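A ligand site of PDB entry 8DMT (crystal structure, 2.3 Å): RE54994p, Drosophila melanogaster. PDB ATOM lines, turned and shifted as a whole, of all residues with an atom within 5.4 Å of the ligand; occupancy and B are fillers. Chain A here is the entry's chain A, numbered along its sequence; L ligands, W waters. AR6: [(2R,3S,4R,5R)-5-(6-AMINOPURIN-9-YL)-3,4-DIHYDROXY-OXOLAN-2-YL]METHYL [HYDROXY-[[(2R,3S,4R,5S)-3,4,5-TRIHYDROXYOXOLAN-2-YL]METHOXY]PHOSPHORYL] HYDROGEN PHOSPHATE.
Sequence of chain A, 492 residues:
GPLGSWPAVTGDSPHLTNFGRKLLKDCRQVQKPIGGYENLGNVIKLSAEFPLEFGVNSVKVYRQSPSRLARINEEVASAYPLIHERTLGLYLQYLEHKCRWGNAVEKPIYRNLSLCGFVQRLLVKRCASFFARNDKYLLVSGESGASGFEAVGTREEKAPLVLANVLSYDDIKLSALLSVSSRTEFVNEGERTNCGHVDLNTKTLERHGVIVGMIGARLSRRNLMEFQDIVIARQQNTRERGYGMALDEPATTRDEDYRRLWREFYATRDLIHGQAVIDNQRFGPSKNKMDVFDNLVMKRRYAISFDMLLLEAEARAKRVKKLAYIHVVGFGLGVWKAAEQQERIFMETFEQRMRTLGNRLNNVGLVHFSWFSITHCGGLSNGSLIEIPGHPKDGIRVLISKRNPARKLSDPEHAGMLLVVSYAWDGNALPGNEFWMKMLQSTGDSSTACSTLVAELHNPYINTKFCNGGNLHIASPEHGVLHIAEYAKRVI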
ATOM      1  N   PHE A 130      15.374  29.201 -13.450  1.00  0.00           N
ATOM      2  CA  PHE A 130      15.525  29.363 -12.004  1.00  0.00           C
ATOM      3  C   PHE A 130      15.858  27.976 -11.450  1.00  0.00           C
ATOM      4  O   PHE A 130      14.959  27.156 -11.221  1.00  0.00           O
ATOM      5  CB  PHE A 130      14.251  29.918 -11.376  1.00  0.00           C
ATOM      6  CG  PHE A 130      14.340  30.134  -9.898  1.00  0.00           C
ATOM      7  CD1 PHE A 130      14.935  31.270  -9.380  1.00  0.00           C
ATOM      8  CD2 PHE A 130      13.817  29.200  -9.015  1.00  0.00           C
ATOM      9  CE1 PHE A 130      15.020  31.474  -8.008  1.00  0.00           C
ATOM     10  CE2 PHE A 130      13.895  29.391  -7.643  1.00  0.00           C
ATOM     11  CZ  PHE A 130      14.498  30.531  -7.146  1.00  0.00           C
ATOM     12  N   PHE A 131      17.151  27.726 -11.225  1.00  0.00           N
ATOM     13  CA  PHE A 131      17.620  26.400 -10.870  1.00  0.00           C
ATOM     14  C   PHE A 131      18.840  26.519  -9.957  1.00  0.00           C
ATOM     15  O   PHE A 131      19.291  27.617  -9.631  1.00  0.00           O
ATOM     16  CB  PHE A 131      17.929  25.573 -12.126  1.00  0.00           C
ATOM     17  CG  PHE A 131      19.034  26.154 -12.966  1.00  0.00           C
ATOM     18  CD1 PHE A 131      18.788  27.225 -13.822  1.00  0.00           C
ATOM     19  CD2 PHE A 131      20.312  25.630 -12.911  1.00  0.00           C
ATOM     20  CE1 PHE A 131      19.801  27.757 -14.594  1.00  0.00           C
ATOM     21  CE2 PHE A 131      21.330  26.159 -13.692  1.00  0.00           C
ATOM     22  CZ  PHE A 131      21.067  27.222 -14.531  1.00  0.00           C
ATOM     23  N   ARG A 192      16.434  11.926 -22.061  1.00  0.00           N
ATOM     24  CA  ARG A 192      17.067  13.105 -21.461  1.00  0.00           C
ATOM     25  C   ARG A 192      18.087  13.746 -22.403  1.00  0.00           C
ATOM     26  O   ARG A 192      18.225  14.965 -22.435  1.00  0.00           O
ATOM     27  CB  ARG A 192      17.728  12.732 -20.130  1.00  0.00           C
ATOM     28  CG  ARG A 192      18.373  13.912 -19.429  1.00  0.00           C
ATOM     29  CD  ARG A 192      18.337  13.779 -17.915  1.00  0.00           C
ATOM     30  NE  ARG A 192      16.968  13.688 -17.400  1.00  0.00           N
ATOM     31  CZ  ARG A 192      16.632  13.912 -16.135  1.00  0.00           C
ATOM     32  NH1 ARG A 192      17.571  14.249 -15.256  1.00  0.00           N
ATOM     33  NH2 ARG A 192      15.372  13.791 -15.751  1.00  0.00           N
ATOM     34  N   GLY A 216       7.766  18.819  -7.934  1.00  0.00           N
ATOM     35  CA  GLY A 216       8.038  18.164  -6.679  1.00  0.00           C
ATOM     36  C   GLY A 216       8.276  19.156  -5.556  1.00  0.00           C
ATOM     37  O   GLY A 216       8.125  20.377  -5.708  1.00  0.00           O
ATOM     38  N   VAL A 329       6.698  10.183 -13.922  1.00  0.00           N
ATOM     39  CA  VAL A 329       8.076  10.410 -13.506  1.00  0.00           C
ATOM     40  C   VAL A 329       8.077  10.773 -12.025  1.00  0.00           C
ATOM     41  O   VAL A 329       7.093  11.256 -11.470  1.00  0.00           O
ATOM     42  CB  VAL A 329       8.771  11.504 -14.346  1.00  0.00           C
ATOM     43  CG1 VAL A 329       8.757  11.140 -15.822  1.00  0.00           C
ATOM     44  CG2 VAL A 329       8.101  12.860 -14.112  1.00  0.00           C
ATOM     45  N   GLY A 330       9.210  10.535 -11.385  1.00  0.00           N
ATOM     46  CA  GLY A 330       9.358  10.865  -9.987  1.00  0.00           C
ATOM     47  C   GLY A 330       9.740  12.315  -9.763  1.00  0.00           C
ATOM     48  O   GLY A 330      10.907  12.609  -9.465  1.00  0.00           O
ATOM     49  N   PHE A 331       8.792  13.230  -9.925  1.00  0.00           N
ATOM     50  CA  PHE A 331       9.074  14.635  -9.724  1.00  0.00           C
ATOM     51  C   PHE A 331       9.397  14.894  -8.253  1.00  0.00           C
ATOM     52  O   PHE A 331       8.668  14.456  -7.365  1.00  0.00           O
ATOM     53  CB  PHE A 331       7.903  15.506 -10.181  1.00  0.00           C
ATOM     54  CG  PHE A 331       6.547  14.952  -9.851  1.00  0.00           C
ATOM     55  CD1 PHE A 331       5.888  14.113 -10.738  1.00  0.00           C
ATOM     56  CD2 PHE A 331       5.918  15.283  -8.667  1.00  0.00           C
ATOM     57  CE1 PHE A 331       4.634  13.611 -10.447  1.00  0.00           C
ATOM     58  CE2 PHE A 331       4.660  14.784  -8.367  1.00  0.00           C
ATOM     59  CZ  PHE A 331       4.022  13.949  -9.255  1.00  0.00           C
ATOM     60  N   GLY A 332      10.493  15.610  -8.018  1.00  0.00           N
ATOM     61  CA  GLY A 332      11.024  15.782  -6.687  1.00  0.00           C
ATOM     62  C   GLY A 332      11.992  14.712  -6.244  1.00  0.00           C
ATOM     63  O   GLY A 332      12.654  14.878  -5.217  1.00  0.00           O
ATOM     64  N   LEU A 333      12.091  13.606  -6.986  1.00  0.00           N
ATOM     65  CA  LEU A 333      12.973  12.501  -6.631  1.00  0.00           C
ATOM     66  C   LEU A 333      14.293  12.532  -7.396  1.00  0.00           C
ATOM     67  O   LEU A 333      15.148  11.671  -7.160  1.00  0.00           O
ATOM     68  CB  LEU A 333      12.260  11.168  -6.889  1.00  0.00           C
ATOM     69  CG  LEU A 333      10.856  11.022  -6.296  1.00  0.00           C
ATOM     70  CD1 LEU A 333      10.272   9.657  -6.624  1.00  0.00           C
ATOM     71  CD2 LEU A 333      10.880  11.262  -4.803  1.00  0.00           C
ATOM     72  N   GLY A 334      14.476  13.485  -8.303  1.00  0.00           N
ATOM     73  CA  GLY A 334      15.718  13.603  -9.030  1.00  0.00           C
ATOM     74  C   GLY A 334      16.739  14.446  -8.290  1.00  0.00           C
ATOM     75  O   GLY A 334      17.239  14.036  -7.244  1.00  0.00           O
ATOM     76  N   VAL A 335      17.046  15.625  -8.832  1.00  0.00           N
ATOM     77  CA  VAL A 335      17.982  16.536  -8.173  1.00  0.00           C
ATOM     78  C   VAL A 335      17.408  17.154  -6.917  1.00  0.00           C
ATOM     79  O   VAL A 335      18.153  17.787  -6.149  1.00  0.00           O
ATOM     80  CB  VAL A 335      18.434  17.648  -9.146  1.00  0.00           C
ATOM     81  CG1 VAL A 335      18.897  17.045 -10.459  1.00  0.00           C
ATOM     82  CG2 VAL A 335      17.307  18.636  -9.373  1.00  0.00           C
ATOM     83  N   TRP A 336      16.113  16.989  -6.672  1.00  0.00           N
ATOM     84  CA  TRP A 336      15.446  17.585  -5.525  1.00  0.00           C
ATOM     85  C   TRP A 336      15.211  16.608  -4.379  1.00  0.00           C
ATOM     86  O   TRP A 336      14.616  16.987  -3.367  1.00  0.00           O
ATOM     87  CB  TRP A 336      14.101  18.194  -5.951  1.00  0.00           C
ATOM     88  CG  TRP A 336      14.206  19.600  -6.446  1.00  0.00           C
ATOM     89  CD1 TRP A 336      15.341  20.340  -6.575  1.00  0.00           C
ATOM     90  CD2 TRP A 336      13.119  20.428  -6.867  1.00  0.00           C
ATOM     91  NE1 TRP A 336      15.028  21.591  -7.069  1.00  0.00           N
ATOM     92  CE2 TRP A 336      13.678  21.670  -7.244  1.00  0.00           C
ATOM     93  CE3 TRP A 336      11.733  20.257  -6.958  1.00  0.00           C
ATOM     94  CZ2 TRP A 336      12.896  22.727  -7.718  1.00  0.00           C
ATOM     95  CZ3 TRP A 336      10.963  21.299  -7.420  1.00  0.00           C
ATOM     96  CH2 TRP A 336      11.540  22.525  -7.794  1.00  0.00           C
ATOM     97  N   LYS A 337      15.648  15.358  -4.515  1.00  0.00           N
ATOM     98  CA  LYS A 337      15.403  14.370  -3.468  1.00  0.00           C
ATOM     99  C   LYS A 337      16.156  14.773  -2.192  1.00  0.00           C
ATOM    100  O   LYS A 337      17.288  15.253  -2.251  1.00  0.00           O
ATOM    101  CB  LYS A 337      15.805  12.976  -3.930  1.00  0.00           C
ATOM    102  CG  LYS A 337      17.252  12.579  -3.694  1.00  0.00           C
ATOM    103  CD  LYS A 337      17.457  11.090  -3.923  1.00  0.00           C
ATOM    104  CE  LYS A 337      16.713  10.256  -2.886  1.00  0.00           C
ATOM    105  NZ  LYS A 337      16.847   8.795  -3.140  1.00  0.00           N
ATOM    106  N   SER A 370       8.281   5.323 -14.568  1.00  0.00           N
ATOM    107  CA  SER A 370       9.528   5.256 -15.312  1.00  0.00           C
ATOM    108  C   SER A 370      10.658   5.871 -14.517  1.00  0.00           C
ATOM    109  O   SER A 370      10.493   6.933 -13.897  1.00  0.00           O
ATOM    110  CB  SER A 370       9.397   5.959 -16.665  1.00  0.00           C
ATOM    111  OG  SER A 370      10.621   5.935 -17.375  1.00  0.00           O
ATOM    112  N   TRP A 371      11.819   5.208 -14.540  1.00  0.00           N
ATOM    113  CA  TRP A 371      13.022   5.653 -13.846  1.00  0.00           C
ATOM    114  C   TRP A 371      12.788   5.761 -12.335  1.00  0.00           C
ATOM    115  O   TRP A 371      13.076   6.772 -11.700  1.00  0.00           O
ATOM    116  CB  TRP A 371      13.539   6.973 -14.412  1.00  0.00           C
ATOM    117  CG  TRP A 371      14.411   6.782 -15.612  1.00  0.00           C
ATOM    118  CD1 TRP A 371      14.008   6.499 -16.885  1.00  0.00           C
ATOM    119  CD2 TRP A 371      15.844   6.853 -15.657  1.00  0.00           C
ATOM    120  NE1 TRP A 371      15.095   6.379 -17.720  1.00  0.00           N
ATOM    121  CE2 TRP A 371      16.235   6.602 -16.989  1.00  0.00           C
ATOM    122  CE3 TRP A 371      16.826   7.113 -14.695  1.00  0.00           C
ATOM    123  CZ2 TRP A 371      17.566   6.593 -17.379  1.00  0.00           C
ATOM    124  CZ3 TRP A 371      18.147   7.109 -15.093  1.00  0.00           C
ATOM    125  CH2 TRP A 371      18.516   6.853 -16.425  1.00  0.00           C
ATOM    126  N   ALA A 424       8.933  16.724 -14.642  1.00  0.00           N
ATOM    127  CA  ALA A 424       9.318  17.460 -13.445  1.00  0.00           C
ATOM    128  C   ALA A 424       9.580  18.920 -13.793  1.00  0.00           C
ATOM    129  O   ALA A 424      10.493  19.225 -14.573  1.00  0.00           O
ATOM    130  CB  ALA A 424      10.546  16.827 -12.795  1.00  0.00           C
ATOM    131  N   TRP A 425       8.785  19.822 -13.221  1.00  0.00           N
ATOM    132  CA  TRP A 425       8.825  21.234 -13.530  1.00  0.00           C
ATOM    133  C   TRP A 425       9.335  22.026 -12.324  1.00  0.00           C
ATOM    134  O   TRP A 425       9.803  21.467 -11.327  1.00  0.00           O
ATOM    135  CB  TRP A 425       7.439  21.698 -13.988  1.00  0.00           C
ATOM    136  CG  TRP A 425       7.427  23.007 -14.727  1.00  0.00           C
ATOM    137  CD1 TRP A 425       8.482  23.611 -15.352  1.00  0.00           C
ATOM    138  CD2 TRP A 425       6.297  23.870 -14.908  1.00  0.00           C
ATOM    139  NE1 TRP A 425       8.076  24.798 -15.917  1.00  0.00           N
ATOM    140  CE2 TRP A 425       6.742  24.984 -15.661  1.00  0.00           C
ATOM    141  CE3 TRP A 425       4.957  23.821 -14.519  1.00  0.00           C
ATOM    142  CZ2 TRP A 425       5.892  26.025 -16.026  1.00  0.00           C
ATOM    143  CZ3 TRP A 425       4.114  24.851 -14.890  1.00  0.00           C
ATOM    144  CH2 TRP A 425       4.587  25.943 -15.631  1.00  0.00           C
ATOM    145  N   ASP A 426       9.232  23.349 -12.418  1.00  0.00           N
ATOM    146  CA  ASP A 426       9.652  24.275 -11.373  1.00  0.00           C
ATOM    147  C   ASP A 426       8.588  25.354 -11.232  1.00  0.00           C
ATOM    148  O   ASP A 426       8.006  25.788 -12.225  1.00  0.00           O
ATOM    149  CB  ASP A 426      11.013  24.904 -11.685  1.00  0.00           C
ATOM    150  CG  ASP A 426      11.598  25.668 -10.511  1.00  0.00           C
ATOM    151  OD1 ASP A 426      10.927  26.579  -9.988  1.00  0.00           O
ATOM    152  OD2 ASP A 426      12.743  25.347 -10.103  1.00  0.00           O
ATOM    153  N   ALA A 429       9.827  28.950 -12.985  1.00  0.00           N
ATOM    154  CA  ALA A 429      10.509  28.877 -14.269  1.00  0.00           C
ATOM    155  C   ALA A 429       9.500  28.577 -15.366  1.00  0.00           C
ATOM    156  O   ALA A 429       8.487  27.917 -15.141  1.00  0.00           O
ATOM    157  CB  ALA A 429      11.615  27.815 -14.260  1.00  0.00           C
ATOM    158  N   ASN A 433      12.990  25.523 -18.022  1.00  0.00           N
ATOM    159  CA  ASN A 433      13.862  26.089 -17.007  1.00  0.00           C
ATOM    160  C   ASN A 433      15.218  26.449 -17.592  1.00  0.00           C
ATOM    161  O   ASN A 433      15.341  27.398 -18.367  1.00  0.00           O
ATOM    162  CB  ASN A 433      14.019  25.130 -15.830  1.00  0.00           C
ATOM    163  CG  ASN A 433      14.452  25.825 -14.547  1.00  0.00           C
ATOM    164  OD1 ASN A 433      15.028  26.913 -14.585  1.00  0.00           O
ATOM    165  ND2 ASN A 433      14.162  25.207 -13.414  1.00  0.00           N
ATOM    166  N   GLU A 434      16.255  25.669 -17.238  1.00  0.00           N
ATOM    167  CA  GLU A 434      17.589  25.889 -17.773  1.00  0.00           C
ATOM    168  C   GLU A 434      17.665  25.710 -19.285  1.00  0.00           C
ATOM    169  O   GLU A 434      18.699  26.008 -19.885  1.00  0.00           O
ATOM    170  CB  GLU A 434      18.580  24.932 -17.099  1.00  0.00           C
ATOM    171  CG  GLU A 434      18.367  23.470 -17.448  1.00  0.00           C
ATOM    172  CD  GLU A 434      17.589  22.732 -16.374  1.00  0.00           C
ATOM    173  OE1 GLU A 434      17.724  21.488 -16.296  1.00  0.00           O
ATOM    174  OE2 GLU A 434      16.833  23.384 -15.627  1.00  0.00           O
ATOM    175  N   THR A 443      18.159  18.174 -16.776  1.00  0.00           N
ATOM    176  CA  THR A 443      17.022  17.665 -16.011  1.00  0.00           C
ATOM    177  C   THR A 443      15.925  17.240 -16.981  1.00  0.00           C
ATOM    178  O   THR A 443      16.050  17.405 -18.203  1.00  0.00           O
ATOM    179  CB  THR A 443      16.474  18.700 -15.022  1.00  0.00           C
ATOM    180  OG1 THR A 443      15.998  19.852 -15.738  1.00  0.00           O
ATOM    181  CG2 THR A 443      17.527  19.121 -14.005  1.00  0.00           C
ATOM    182  N   GLY A 444      14.846  16.689 -16.432  1.00  0.00           N
ATOM    183  CA  GLY A 444      13.674  16.395 -17.233  1.00  0.00           C
ATOM    184  C   GLY A 444      12.938  17.634 -17.695  1.00  0.00           C
ATOM    185  O   GLY A 444      12.209  17.564 -18.693  1.00  0.00           O
ATOM    186  N   ASP A 445      13.115  18.755 -16.999  1.00  0.00           N
ATOM    187  CA  ASP A 445      12.509  20.007 -17.425  1.00  0.00           C
ATOM    188  C   ASP A 445      13.074  20.460 -18.769  1.00  0.00           C
ATOM    189  O   ASP A 445      12.320  20.726 -19.719  1.00  0.00           O
ATOM    190  CB  ASP A 445      12.737  21.091 -16.369  1.00  0.00           C
ATOM    191  CG  ASP A 445      11.616  22.105 -16.325  1.00  0.00           C
ATOM    192  OD1 ASP A 445      10.978  22.338 -17.367  1.00  0.00           O
ATOM    193  OD2 ASP A 445      11.398  22.691 -15.247  1.00  0.00           O
HETATM  194  N1  AR6 L   1      16.461   9.798 -17.733  1.00  0.00           N
HETATM  195  C2  AR6 L   1      15.218   9.762 -17.208  1.00  0.00           C
HETATM  196  N3  AR6 L   1      14.832  10.020 -15.969  1.00  0.00           N
HETATM  197  C4  AR6 L   1      15.878  10.360 -15.195  1.00  0.00           C
HETATM  198  C5  AR6 L   1      17.193  10.438 -15.583  1.00  0.00           C
HETATM  199  C6  AR6 L   1      17.492  10.146 -16.934  1.00  0.00           C
HETATM  200  N6  AR6 L   1      18.717  10.182 -17.445  1.00  0.00           N
HETATM  201  N7  AR6 L   1      17.990  10.820 -14.513  1.00  0.00           N
HETATM  202  C8  AR6 L   1      17.148  10.959 -13.507  1.00  0.00           C
HETATM  203  N9  AR6 L   1      15.851  10.683 -13.873  1.00  0.00           N
HETATM  204  PA  AR6 L   1      14.519  15.764 -12.180  1.00  0.00           P
HETATM  205  PB  AR6 L   1      13.186  16.969  -9.852  1.00  0.00           P
HETATM  206  C1' AR6 L   1      14.666  10.733 -13.017  1.00  0.00           C
HETATM  207  O1A AR6 L   1      14.328  16.056 -13.632  1.00  0.00           O
HETATM  208  O1B AR6 L   1      13.990  16.094  -8.952  1.00  0.00           O
HETATM  209  C1D AR6 L   1      14.724  21.149 -12.877  1.00  0.00           C
HETATM  210  O1D AR6 L   1      15.608  22.158 -13.203  1.00  0.00           O
HETATM  211  C2' AR6 L   1      14.930  10.989 -11.544  1.00  0.00           C
HETATM  212  O2' AR6 L   1      15.462   9.873 -10.854  1.00  0.00           O
HETATM  213  O2A AR6 L   1      15.805  16.160 -11.544  1.00  0.00           O
HETATM  214  O2B AR6 L   1      11.734  17.158  -9.546  1.00  0.00           O
HETATM  215  C2D AR6 L   1      13.314  21.744 -12.660  1.00  0.00           C
HETATM  216  O2D AR6 L   1      12.998  22.864 -13.463  1.00  0.00           O
HETATM  217  C3' AR6 L   1      13.526  11.405 -11.095  1.00  0.00           C
HETATM  218  O3' AR6 L   1      12.739  10.239 -10.883  1.00  0.00           O
HETATM  219  O3A AR6 L   1      13.313  16.425 -11.363  1.00  0.00           O
HETATM  220  C3D AR6 L   1      13.288  21.985 -11.161  1.00  0.00           C
HETATM  221  O3D AR6 L   1      14.047  23.144 -10.816  1.00  0.00           O
HETATM  222  C4' AR6 L   1      12.993  12.180 -12.309  1.00  0.00           C
HETATM  223  O4' AR6 L   1      13.885  11.836 -13.408  1.00  0.00           O
HETATM  224  C4D AR6 L   1      14.004  20.716 -10.678  1.00  0.00           C
HETATM  225  O4D AR6 L   1      15.080  20.547 -11.624  1.00  0.00           O
HETATM  226  C5' AR6 L   1      12.929  13.679 -12.191  1.00  0.00           C
HETATM  227  O5' AR6 L   1      14.259  14.200 -11.921  1.00  0.00           O
HETATM  228  C5D AR6 L   1      13.166  19.467 -10.663  1.00  0.00           C
HETATM  229  O5D AR6 L   1      13.887  18.407  -9.975  1.00  0.00           O
HETATM  230  O   HOH W   1      19.369   8.884 -20.084  1.00  0.00           O
HETATM  231  O   HOH W   2      17.547  14.367 -12.591  1.00  0.00           O
HETATM  232  O   HOH W   3      16.333   9.495 -20.434  1.00  0.00           O
HETATM  233  O   HOH W   4      13.077  18.554 -14.159  1.00  0.00           O
HETATM  234  O   HOH W   5       9.566  19.044  -9.948  1.00  0.00           O
HETATM  235  O   HOH W   6      12.029  10.191 -15.539  1.00  0.00           O
HETATM  236  O   HOH W   7      11.354   9.308 -13.117  1.00  0.00           O
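O of Gly 330 lies close to O3' of the ligand, at 3.3 Å.
O2B of the ligand lies within hydrogen-bond range of N of Gly 332.
OD2 of Asp 445 lies within hydrogen-bond range of O2D of the ligand, 2.4 Å away.
N of Val 335 is in hydrogen-bond range of O2A of the ligand, 3.0 Å away.
The backbone NH (N) of Gly 334 sits at hydrogen-bond distance from an oxygen (O1B) of the ligand (2.7 Å).
N of Trp 336 lies within hydrogen-bond range of O1B of the ligand (3.2 Å).
The guanidinium group of Arg 192 is in salt-bridge range of an oxygen (O1A) of the ligand, 3.3 Å away.
ND2 of Asn 433 sits at hydrogen-bond distance from O2D of the ligand, at 2.6 Å.
N of Gly 444 sits at hydrogen-bond distance from O1A of the ligand (2.9 Å).
OG1 of Thr 443 sits close to O1D of the ligand (3.4 Å).
OE2 of Glu 434 sits at hydrogen-bond distance from O1D of the ligand (3.0 Å).
An oxygen (O3D) of the ligand is in hydrogen-bond range of the side-chain carboxylate (OD2) of Asp 426 (2.7 Å).
OD1 of Asn 433 sits at hydrogen-bond distance from N of Phe 130 (2.6 Å).
The side-chain carboxylate of Glu 434 lies within hydrogen-bond range of the side-chain hydroxyl of Thr 443, 2.4 Å away.
The backbone NH of Lys 337 is in hydrogen-bond range of the backbone carbonyl oxygen of Gly 332 (3.1 Å).
The indole nitrogen of Trp 425 lies within hydrogen-bond range of the backbone carbonyl oxygen of Ala 429 (3.2 Å).
The side-chain hydroxyl (OG1) of Thr 443 lies close to the backbone NH (N) of Asp 445, 3.3 Å away.
Phe 331 touches the ligand (C to O2B, 3.5 Å).
N of Leu 333 touches O1B of the ligand, at 3.7 Å.
Trp 371 touches the ligand.
Ala 424 touches the ligand (CB to O3A, 3.1 Å).
O of Trp 425 touches C3D of the ligand (3.5 Å).
Hydrophobic or aromatic side chains that line the ligand: Val 335, Trp 336, Trp 371 and Ala 424.
The nearest printed residue that does not touch the ligand is Phe 130 (4.1 Å).
Water W2 lies within hydrogen-bond range of the guanidinium group of Arg 192 and an oxygen (O2A) of the ligand.
Water W3 lies within hydrogen-bond range of a nitrogen (N1) of the ligand (2.7 Å) and the backbone NH of Arg 192 (2.9 Å).
Water W7 lies within hydrogen-bond range of the backbone carbonyl oxygen of Ser 370 (2.6 Å), an oxygen (O3') of the ligand (2.8 Å), the backbone NH of Gly 330 (3.0 Å) and the backbone carbonyl oxygen of Trp 371 (3.4 Å).
Water W4 lies within hydrogen-bond range of the backbone carbonyl oxygen (O) of Ala 424 (2.7 Å), an oxygen (O1A) of the ligand (2.8 Å), the backbone NH (N) of Asp 445 (2.8 Å) and the backbone NH (N) of Gly 444 (3.4 Å).
Water W5 lies within hydrogen-bond range of N of Gly 216, O of Trp 425 and O2B of the ligand.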
